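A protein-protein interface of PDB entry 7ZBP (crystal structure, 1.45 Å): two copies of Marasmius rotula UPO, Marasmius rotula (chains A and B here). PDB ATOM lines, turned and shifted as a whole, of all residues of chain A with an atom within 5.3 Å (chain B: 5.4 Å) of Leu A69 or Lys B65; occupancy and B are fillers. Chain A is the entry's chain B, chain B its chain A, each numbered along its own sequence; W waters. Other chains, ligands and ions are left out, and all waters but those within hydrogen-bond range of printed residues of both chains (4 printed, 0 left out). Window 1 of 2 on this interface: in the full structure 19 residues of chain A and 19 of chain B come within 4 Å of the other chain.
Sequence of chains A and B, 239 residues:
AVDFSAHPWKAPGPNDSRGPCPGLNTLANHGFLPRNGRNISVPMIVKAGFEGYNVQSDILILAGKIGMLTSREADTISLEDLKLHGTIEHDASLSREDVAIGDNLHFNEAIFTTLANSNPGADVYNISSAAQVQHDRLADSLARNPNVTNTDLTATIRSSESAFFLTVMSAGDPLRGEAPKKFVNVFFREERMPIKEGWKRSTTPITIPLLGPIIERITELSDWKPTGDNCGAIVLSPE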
ATOM      1  N   LYS A  65       0.557   6.564 -13.606  1.00  0.00           N
ATOM      2  CA  LYS A  65       1.133   6.946 -14.925  1.00  0.00           C
ATOM      3  C   LYS A  65       0.436   8.192 -15.444  1.00  0.00           C
ATOM      4  O   LYS A  65       1.082   9.002 -16.103  1.00  0.00           O
ATOM      5  CB  LYS A  65       1.112   5.781 -15.893  1.00  0.00           C
ATOM      6  CG  LYS A  65       2.138   4.722 -15.518  1.00  0.00           C
ATOM      7  CD  LYS A  65       2.412   3.693 -16.588  1.00  0.00           C
ATOM      8  CE  LYS A  65       1.200   2.934 -16.913  1.00  0.00           C
ATOM      9  NZ  LYS A  65       1.504   1.883 -17.910  1.00  0.00           N
ATOM     10  N   ILE A  66      -0.851   8.368 -15.183  1.00  0.00           N
ATOM     11  CA  ILE A  66      -1.531   9.625 -15.554  1.00  0.00           C
ATOM     12  C   ILE A  66      -0.946  10.782 -14.728  1.00  0.00           C
ATOM     13  O   ILE A  66      -0.632  11.843 -15.266  1.00  0.00           O
ATOM     14  CB  ILE A  66      -3.057   9.488 -15.407  1.00  0.00           C
ATOM     15  CG1 ILE A  66      -3.604   8.410 -16.332  1.00  0.00           C
ATOM     16  CG2 ILE A  66      -3.734  10.818 -15.667  1.00  0.00           C
ATOM     17  CD1 ILE A  66      -5.020   8.064 -15.959  1.00  0.00           C
ATOM     18  N   GLY A  67      -0.729  10.578 -13.418  1.00  0.00           N
ATOM     19  CA  GLY A  67      -0.143  11.639 -12.600  1.00  0.00           C
ATOM     20  C   GLY A  67       1.263  12.024 -13.031  1.00  0.00           C
ATOM     21  O   GLY A  67       1.644  13.209 -12.879  1.00  0.00           O
ATOM     22  N   MET A  68       2.043  11.079 -13.551  1.00  0.00           N
ATOM     23  CA  MET A  68       3.423  11.385 -13.984  1.00  0.00           C
ATOM     24  C   MET A  68       3.408  12.459 -15.081  1.00  0.00           C
ATOM     25  O   MET A  68       4.427  13.135 -15.239  1.00  0.00           O
ATOM     26  CB  MET A  68       4.138  10.166 -14.551  1.00  0.00           C
ATOM     27  CG  MET A  68       4.414   9.023 -13.575  1.00  0.00           C
ATOM     28  SD  MET A  68       5.552   9.464 -12.220  1.00  0.00           S
ATOM     29  CE  MET A  68       4.467   9.517 -10.819  1.00  0.00           C
ATOM     30  N   LEU A  69       2.300  12.574 -15.826  1.00  0.00           N
ATOM     31  CA  LEU A  69       2.247  13.570 -16.937  1.00  0.00           C
ATOM     32  C   LEU A  69       2.362  14.968 -16.382  1.00  0.00           C
ATOM     33  O   LEU A  69       2.729  15.888 -17.151  1.00  0.00           O
ATOM     34  CB  LEU A  69       0.920  13.454 -17.702  1.00  0.00           C
ATOM     35  CG  LEU A  69       0.575  12.089 -18.269  1.00  0.00           C
ATOM     36  CD1 LEU A  69      -0.819  12.135 -18.871  1.00  0.00           C
ATOM     37  CD2 LEU A  69       1.581  11.666 -19.313  1.00  0.00           C
ATOM     38  N   THR A  70       2.075  15.177 -15.104  1.00  0.00           N
ATOM     39  CA  THR A  70       2.024  16.543 -14.542  1.00  0.00           C
ATOM     40  C   THR A  70       3.393  17.132 -14.293  1.00  0.00           C
ATOM     41  O   THR A  70       3.468  18.374 -14.031  1.00  0.00           O
ATOM     42  CB  THR A  70       1.186  16.590 -13.264  1.00  0.00           C
ATOM     43  OG1 THR A  70       1.802  15.896 -12.192  1.00  0.00           O
ATOM     44  CG2 THR A  70      -0.229  16.118 -13.498  1.00  0.00           C
ATOM     45  N   SER A  71       4.445  16.334 -14.255  1.00  0.00           N
ATOM     46  CA  SER A  71       5.797  16.869 -13.955  1.00  0.00           C
ATOM     47  C   SER A  71       6.590  17.135 -15.242  1.00  0.00           C
ATOM     48  O   SER A  71       6.187  16.672 -16.340  1.00  0.00           O
ATOM     49  CB  SER A  71       6.608  15.958 -13.031  1.00  0.00           C
ATOM     50  OG  SER A  71       7.072  14.886 -13.808  1.00  0.00           O
ATOM     51  N   ARG A  72       7.759  17.717 -15.084  1.00  0.00           N
ATOM     52  CA  ARG A  72       8.747  17.885 -16.153  1.00  0.00           C
ATOM     53  C   ARG A  72       9.818  16.808 -16.120  1.00  0.00           C
ATOM     54  O   ARG A  72      10.779  16.883 -16.921  1.00  0.00           O
ATOM     55  CB  ARG A  72       9.334  19.297 -16.023  1.00  0.00           C
ATOM     56  CG  ARG A  72       8.342  20.381 -16.372  1.00  0.00           C
ATOM     57  CD  ARG A  72       8.968  21.759 -16.157  1.00  0.00           C
ATOM     58  NE  ARG A  72       8.089  22.728 -16.803  1.00  0.00           N
ATOM     59  CZ  ARG A  72       7.053  23.323 -16.232  1.00  0.00           C
ATOM     60  NH1 ARG A  72       6.713  23.056 -14.973  1.00  0.00           N
ATOM     61  NH2 ARG A  72       6.334  24.168 -16.960  1.00  0.00           N
ATOM     62  N   GLU A  73       9.713  15.794 -15.261  1.00  0.00           N
ATOM     63  CA  GLU A  73      10.776  14.824 -15.096  1.00  0.00           C
ATOM     64  C   GLU A  73      10.396  13.514 -15.788  1.00  0.00           C
ATOM     65  O   GLU A  73       9.194  13.224 -16.028  1.00  0.00           O
ATOM     66  CB  GLU A  73      11.080  14.600 -13.615  1.00  0.00           C
ATOM     67  CG  GLU A  73      11.766  15.774 -12.948  1.00  0.00           C
ATOM     68  CD  GLU A  73      10.871  16.935 -12.663  1.00  0.00           C
ATOM     69  OE1 GLU A  73       9.853  16.719 -11.971  1.00  0.00           O
ATOM     70  OE2 GLU A  73      11.167  18.077 -13.136  1.00  0.00           O
ATOM     71  N   ALA A  74      11.396  12.692 -16.047  1.00  0.00           N
ATOM     72  CA  ALA A  74      11.231  11.494 -16.904  1.00  0.00           C
ATOM     73  C   ALA A  74      10.321  10.436 -16.276  1.00  0.00           C
ATOM     74  O   ALA A  74       9.582   9.799 -17.003  1.00  0.00           O
ATOM     75  CB  ALA A  74      12.588  10.933 -17.215  1.00  0.00           C
ATOM     76  N   ASP A  75      10.394  10.208 -14.958  1.00  0.00           N
ATOM     77  CA  ASP A  75       9.688   9.062 -14.342  1.00  0.00           C
ATOM     78  C   ASP A  75       9.336   9.336 -12.883  1.00  0.00           C
ATOM     79  O   ASP A  75       9.065   8.375 -12.157  1.00  0.00           O
ATOM     80  CB  ASP A  75      10.459   7.737 -14.470  1.00  0.00           C
ATOM     81  CG  ASP A  75      11.706   7.537 -13.628  1.00  0.00           C
ATOM     82  OD1 ASP A  75      12.291   8.552 -13.182  1.00  0.00           O
ATOM     83  OD2 ASP A  75      12.028   6.356 -13.341  1.00  0.00           O
ATOM     84  N   THR A  76       9.320  10.588 -12.516  1.00  0.00           N
ATOM     85  CA  THR A  76       8.962  10.994 -11.136  1.00  0.00           C
ATOM     86  C   THR A  76       8.129  12.262 -11.159  1.00  0.00           C
ATOM     87  O   THR A  76       8.165  13.007 -12.160  1.00  0.00           O
ATOM     88  CB  THR A  76      10.178  11.217 -10.241  1.00  0.00           C
ATOM     89  OG1 THR A  76      10.995  12.273 -10.796  1.00  0.00           O
ATOM     90  CG2 THR A  76      10.966   9.951 -10.029  1.00  0.00           C
ATOM     91  N   LEU A  84      -1.746  20.328 -11.294  1.00  0.00           N
ATOM     92  CA  LEU A  84      -1.896  20.747 -12.710  1.00  0.00           C
ATOM     93  C   LEU A  84      -3.366  20.584 -13.121  1.00  0.00           C
ATOM     94  O   LEU A  84      -3.892  19.504 -13.241  1.00  0.00           O
ATOM     95  CB  LEU A  84      -0.953  19.989 -13.627  1.00  0.00           C
ATOM     96  CG  LEU A  84      -1.037  20.378 -15.110  1.00  0.00           C
ATOM     97  CD1 LEU A  84      -0.667  21.858 -15.269  1.00  0.00           C
ATOM     98  CD2 LEU A  84      -0.142  19.496 -15.943  1.00  0.00           C
ATOM     99  N   THR A  87      -5.385  17.607 -15.706  1.00  0.00           N
ATOM    100  CA  THR A  87      -4.829  16.252 -15.887  1.00  0.00           C
ATOM    101  C   THR A  87      -5.697  15.297 -15.056  1.00  0.00           C
ATOM    102  O   THR A  87      -6.636  14.740 -15.556  1.00  0.00           O
ATOM    103  CB  THR A  87      -3.334  16.176 -15.586  1.00  0.00           C
ATOM    104  OG1 THR A  87      -2.653  17.131 -16.408  1.00  0.00           O
ATOM    105  CG2 THR A  87      -2.839  14.782 -15.866  1.00  0.00           C
ATOM    106  N   ILE A 234      -7.597  15.312 -21.471  1.00  0.00           N
ATOM    107  CA  ILE A 234      -6.736  15.700 -20.335  1.00  0.00           C
ATOM    108  C   ILE A 234      -5.580  16.547 -20.849  1.00  0.00           C
ATOM    109  O   ILE A 234      -5.147  16.434 -22.007  1.00  0.00           O
ATOM    110  CB  ILE A 234      -6.247  14.500 -19.518  1.00  0.00           C
ATOM    111  CG1 ILE A 234      -5.320  13.581 -20.305  1.00  0.00           C
ATOM    112  CG2 ILE A 234      -7.399  13.746 -18.905  1.00  0.00           C
ATOM    113  CD1 ILE A 234      -4.403  12.782 -19.392  1.00  0.00           C
ATOM    114  N   VAL A 235      -5.036  17.345 -19.966  1.00  0.00           N
ATOM    115  CA  VAL A 235      -3.785  18.096 -20.133  1.00  0.00           C
ATOM    116  C   VAL A 235      -2.636  17.086 -20.038  1.00  0.00           C
ATOM    117  O   VAL A 235      -2.551  16.353 -19.046  1.00  0.00           O
ATOM    118  CB  VAL A 235      -3.689  19.217 -19.090  1.00  0.00           C
ATOM    119  CG1 VAL A 235      -2.333  19.888 -19.073  1.00  0.00           C
ATOM    120  CG2 VAL A 235      -4.811  20.231 -19.335  1.00  0.00           C
ATOM    121  N   LEU A 236      -1.817  16.993 -21.069  1.00  0.00           N
ATOM    122  CA  LEU A 236      -0.804  15.920 -21.216  1.00  0.00           C
ATOM    123  C   LEU A 236       0.577  16.328 -20.728  1.00  0.00           C
ATOM    124  O   LEU A 236       1.434  15.477 -20.664  1.00  0.00           O
ATOM    125  CB  LEU A 236      -0.774  15.489 -22.694  1.00  0.00           C
ATOM    126  CG  LEU A 236      -2.064  14.866 -23.227  1.00  0.00           C
ATOM    127  CD1 LEU A 236      -1.989  14.741 -24.744  1.00  0.00           C
ATOM    128  CD2 LEU A 236      -2.338  13.543 -22.589  1.00  0.00           C
ATOM    129  N   SER A 237       0.779  17.570 -20.340  1.00  0.00           N
ATOM    130  CA  SER A 237       2.092  18.075 -19.882  1.00  0.00           C
ATOM    131  C   SER A 237       1.893  19.405 -19.207  1.00  0.00           C
ATOM    132  O   SER A 237       0.964  20.145 -19.545  1.00  0.00           O
ATOM    133  CB  SER A 237       3.040  18.153 -21.079  1.00  0.00           C
ATOM    134  OG  SER A 237       4.163  18.969 -20.805  1.00  0.00           O
ATOM    135  N   PRO A 238       2.771  19.811 -18.299  1.00  0.00           N
ATOM    136  CA  PRO A 238       2.757  21.183 -17.815  1.00  0.00           C
ATOM    137  C   PRO A 238       3.286  22.142 -18.902  1.00  0.00           C
ATOM    138  O   PRO A 238       3.693  21.674 -19.918  1.00  0.00           O
ATOM    139  CB  PRO A 238       3.606  21.140 -16.552  1.00  0.00           C
ATOM    140  CG  PRO A 238       4.537  20.001 -16.768  1.00  0.00           C
ATOM    141  CD  PRO A 238       3.804  19.003 -17.643  1.00  0.00           C
ATOM    142  N   VAL B  42      11.159   5.636 -19.831  1.00  0.00           N
ATOM    143  CA  VAL B  42      11.381   7.015 -20.308  1.00  0.00           C
ATOM    144  C   VAL B  42      12.830   7.421 -20.159  1.00  0.00           C
ATOM    145  O   VAL B  42      13.404   7.966 -21.116  1.00  0.00           O
ATOM    146  CB  VAL B  42      10.366   8.009 -19.762  1.00  0.00           C
ATOM    147  CG1 VAL B  42      10.655   9.412 -20.239  1.00  0.00           C
ATOM    148  CG2 VAL B  42       8.981   7.549 -20.156  1.00  0.00           C
ATOM    149  N   LEU B  60      11.275  14.258 -25.324  1.00  0.00           N
ATOM    150  CA  LEU B  60      11.199  12.813 -25.073  1.00  0.00           C
ATOM    151  C   LEU B  60      10.502  12.491 -23.742  1.00  0.00           C
ATOM    152  O   LEU B  60       9.877  11.437 -23.646  1.00  0.00           O
ATOM    153  CB  LEU B  60      12.607  12.255 -25.154  1.00  0.00           C
ATOM    154  CG  LEU B  60      13.251  12.408 -26.540  1.00  0.00           C
ATOM    155  CD1 LEU B  60      14.661  11.914 -26.485  1.00  0.00           C
ATOM    156  CD2 LEU B  60      12.482  11.621 -27.586  1.00  0.00           C
ATOM    157  N   ILE B  61      10.642  13.359 -22.750  1.00  0.00           N
ATOM    158  CA  ILE B  61       9.898  13.174 -21.480  1.00  0.00           C
ATOM    159  C   ILE B  61       8.413  13.356 -21.737  1.00  0.00           C
ATOM    160  O   ILE B  61       7.593  12.539 -21.274  1.00  0.00           O
ATOM    161  CB  ILE B  61      10.438  14.164 -20.441  1.00  0.00           C
ATOM    162  CG1 ILE B  61      11.826  13.762 -19.938  1.00  0.00           C
ATOM    163  CG2 ILE B  61       9.455  14.379 -19.291  1.00  0.00           C
ATOM    164  CD1 ILE B  61      12.519  14.845 -19.140  1.00  0.00           C
ATOM    165  N   LEU B  62       8.051  14.414 -22.465  1.00  0.00           N
ATOM    166  CA  LEU B  62       6.633  14.675 -22.787  1.00  0.00           C
ATOM    167  C   LEU B  62       6.061  13.464 -23.549  1.00  0.00           C
ATOM    168  O   LEU B  62       5.016  12.917 -23.126  1.00  0.00           O
ATOM    169  CB  LEU B  62       6.544  15.949 -23.617  1.00  0.00           C
ATOM    170  CG  LEU B  62       5.144  16.512 -23.876  1.00  0.00           C
ATOM    171  CD1 LEU B  62       5.326  17.981 -24.224  1.00  0.00           C
ATOM    172  CD2 LEU B  62       4.432  15.729 -24.946  1.00  0.00           C
ATOM    173  N   ALA B  63       6.599  13.093 -24.713  1.00  0.00           N
ATOM    174  CA  ALA B  63       6.095  11.978 -25.510  1.00  0.00           C
ATOM    175  C   ALA B  63       6.218  10.661 -24.758  1.00  0.00           C
ATOM    176  O   ALA B  63       5.322   9.818 -24.838  1.00  0.00           O
ATOM    177  CB  ALA B  63       6.843  11.925 -26.818  1.00  0.00           C
ATOM    178  N   GLY B  64       7.371  10.465 -24.112  1.00  0.00           N
ATOM    179  CA  GLY B  64       7.664   9.172 -23.485  1.00  0.00           C
ATOM    180  C   GLY B  64       6.632   8.826 -22.422  1.00  0.00           C
ATOM    181  O   GLY B  64       6.186   7.675 -22.382  1.00  0.00           O
ATOM    182  N   LYS B  65       6.274   9.788 -21.574  1.00  0.00           N
ATOM    183  CA  LYS B  65       5.303   9.491 -20.482  1.00  0.00           C
ATOM    184  C   LYS B  65       3.921   9.203 -21.033  1.00  0.00           C
ATOM    185  O   LYS B  65       3.175   8.423 -20.450  1.00  0.00           O
ATOM    186  CB  LYS B  65       5.324  10.575 -19.437  1.00  0.00           C
ATOM    187  CG  LYS B  65       6.642  10.585 -18.695  1.00  0.00           C
ATOM    188  CD  LYS B  65       6.645  11.528 -17.491  1.00  0.00           C
ATOM    189  CE  LYS B  65       6.295  12.932 -17.878  1.00  0.00           C
ATOM    190  NZ  LYS B  65       6.566  13.897 -16.810  1.00  0.00           N
ATOM    191  N   ILE B  66       3.557   9.821 -22.157  1.00  0.00           N
ATOM    192  CA  ILE B  66       2.279   9.470 -22.813  1.00  0.00           C
ATOM    193  C   ILE B  66       2.396   8.062 -23.350  1.00  0.00           C
ATOM    194  O   ILE B  66       1.439   7.270 -23.171  1.00  0.00           O
ATOM    195  CB  ILE B  66       1.940  10.491 -23.909  1.00  0.00           C
ATOM    196  CG1 ILE B  66       1.847  11.905 -23.312  1.00  0.00           C
ATOM    197  CG2 ILE B  66       0.678  10.054 -24.643  1.00  0.00           C
ATOM    198  CD1 ILE B  66       1.840  12.955 -24.398  1.00  0.00           C
ATOM    199  N   GLY B  67       3.529   7.697 -23.967  1.00  0.00           N
ATOM    200  CA  GLY B  67       3.682   6.330 -24.468  1.00  0.00           C
ATOM    201  C   GLY B  67       3.597   5.279 -23.371  1.00  0.00           C
ATOM    202  O   GLY B  67       3.158   4.149 -23.599  1.00  0.00           O
ATOM    203  N   MET B  68       4.048   5.588 -22.171  1.00  0.00           N
ATOM    204  CA  MET B  68       4.025   4.634 -21.040  1.00  0.00           C
ATOM    205  C   MET B  68       2.587   4.223 -20.720  1.00  0.00           C
ATOM    206  O   MET B  68       2.399   3.150 -20.190  1.00  0.00           O
ATOM    207  CB  MET B  68       4.647   5.267 -19.778  1.00  0.00           C
ATOM    208  CG  MET B  68       6.124   5.503 -19.848  1.00  0.00           C
ATOM    209  SD  MET B  68       7.194   4.061 -20.075  1.00  0.00           S
ATOM    210  CE  MET B  68       7.720   4.277 -21.782  1.00  0.00           C
ATOM    211  N   LEU B  69       1.603   5.068 -21.063  1.00  0.00           N
ATOM    212  CA  LEU B  69       0.185   4.729 -20.808  1.00  0.00           C
ATOM    213  C   LEU B  69      -0.207   3.476 -21.580  1.00  0.00           C
ATOM    214  O   LEU B  69      -1.247   2.876 -21.231  1.00  0.00           O
ATOM    215  CB  LEU B  69      -0.725   5.898 -21.163  1.00  0.00           C
ATOM    216  CG  LEU B  69      -0.461   7.224 -20.472  1.00  0.00           C
ATOM    217  CD1 LEU B  69      -1.287   8.369 -21.070  1.00  0.00           C
ATOM    218  CD2 LEU B  69      -0.646   7.124 -18.968  1.00  0.00           C
HETATM  219  O   HOH W   1       5.024  15.623 -18.872  1.00  0.00           O
HETATM  220  O   HOH W   2       3.156   8.065 -17.723  1.00  0.00           O
HETATM  221  O   HOH W   3      -1.639   2.409 -18.335  1.00  0.00           O
HETATM  222  O   HOH W   4       3.826  14.040 -20.756  1.00  0.00           O
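The backbone carbonyl oxygen (O) of Met B68 is in hydrogen-bond range of the side-chain amino group (NZ) of Lys A65. The side-chain amino group of Lys B65 sits at hydrogen-bond distance from the backbone carbonyl oxygen of Met A68, 2.8 Å away. The side-chain amino group (NZ) of Lys B65 lies within hydrogen-bond range of the backbone carbonyl oxygen (O) of Glu A73, 2.8 Å away. The side-chain amino group of Lys B65 lies within hydrogen-bond range of the backbone carbonyl oxygen of Ser A71 (2.8 Å).
The side-chain hydroxyl (OG) of Ser A71 is in hydrogen-bond range of the backbone NH (N) of Glu A73 (3.1 Å). O of Thr A76 lies within hydrogen-bond range of OG of Ser A71 (2.7 Å). The backbone carbonyl oxygen (O) of Met A68 sits at hydrogen-bond distance from the side-chain hydroxyl (OG) of Ser A71 (3.5 Å).
Among the printed residues, merely in contact across the chains: Lys A65 with Leu B69 (3.8 Å), Ile A66 with Leu B69 (3.99 Å), Leu A69 with Lys B65 (3.8 Å), Leu A69 with Ile B66 (3.9 Å), Arg A72 with Ile B61 (3.5 Å), Glu A73 with Ile B61 (3.5 Å), Ala A74 with Val B42 (3.4 Å), Ala A74 with Ile B61 (3.8 Å), Ala A74 with Lys B65 (3.4 Å) and Ser A237 with Leu B62 (3.7 Å).
Of chain B, only Lys B65 and Ile B66 come within 4 Å of Leu A69. Lys B65 touches five residues of chain A. Printed residues of chain A within 4 Å of Leu B69: Lys A65 (3.8 Å) and Ile A66 (3.99 Å). Printed residues of chain B within 4 Å of Lys A65: Met B68 and Leu B69. Of the printed residues of chain B, Ala A74 touches Val B42 (3.4 Å), Ile B61 (3.8 Å) and Lys B65 (3.4 Å). Of the printed residues of chain B, Ser A237 touches Leu B62. Printed residues of chain B within 4 Å of Met A68: Lys B65 (2.8 Å). Thr A76 touches none of the printed residues of chain B. Gly B67 touches none of the printed residues of chain A. The nearest residue of chain B that does not touch Leu A69 is Leu B69 (4.4 Å). The nearest residue of chain A that does not touch Lys B65 is Arg A72 (4.4 Å).
Hydrophobic or aromatic side chains of chain B that line the printed part of chain A: Val B42, Ile B61, Leu B62 and Leu B69. Hydrophobic or aromatic side chains of chain A within 4 Å of the printed part of chain B: Leu A69 and Ala A74.
Lys A65 touches Met B68, and with the chains exchanged Met A68 touches Lys B65. Lys A65 touches Leu B69, and with the chains exchanged Leu A69 touches Lys B65. Ile A66 touches Leu B69, and with the chains exchanged Leu A69 touches Ile B66. Positions printed for both chains: 65, 66, 67, 68 and 69. Of the 14 pairs that touch across the chains among the printed residues, 6 have their exchanged pair printed and touching as well.
Water W2 lies within hydrogen-bond range of O of Lys B65 and O of Lys A65. Water W4 bridges the backbone carbonyl oxygen of Leu A236 (2.8 Å) and the backbone carbonyl oxygen of Leu B62 (2.9 Å). Water W1 lies within hydrogen-bond range of the backbone carbonyl oxygen of Leu A69, the backbone carbonyl oxygen of Ser A71 and the side-chain amino group of Lys B65. Water W3 bridges O of Leu B69 (3.0 Å) and NZ of Lys A65 (3.2 Å).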
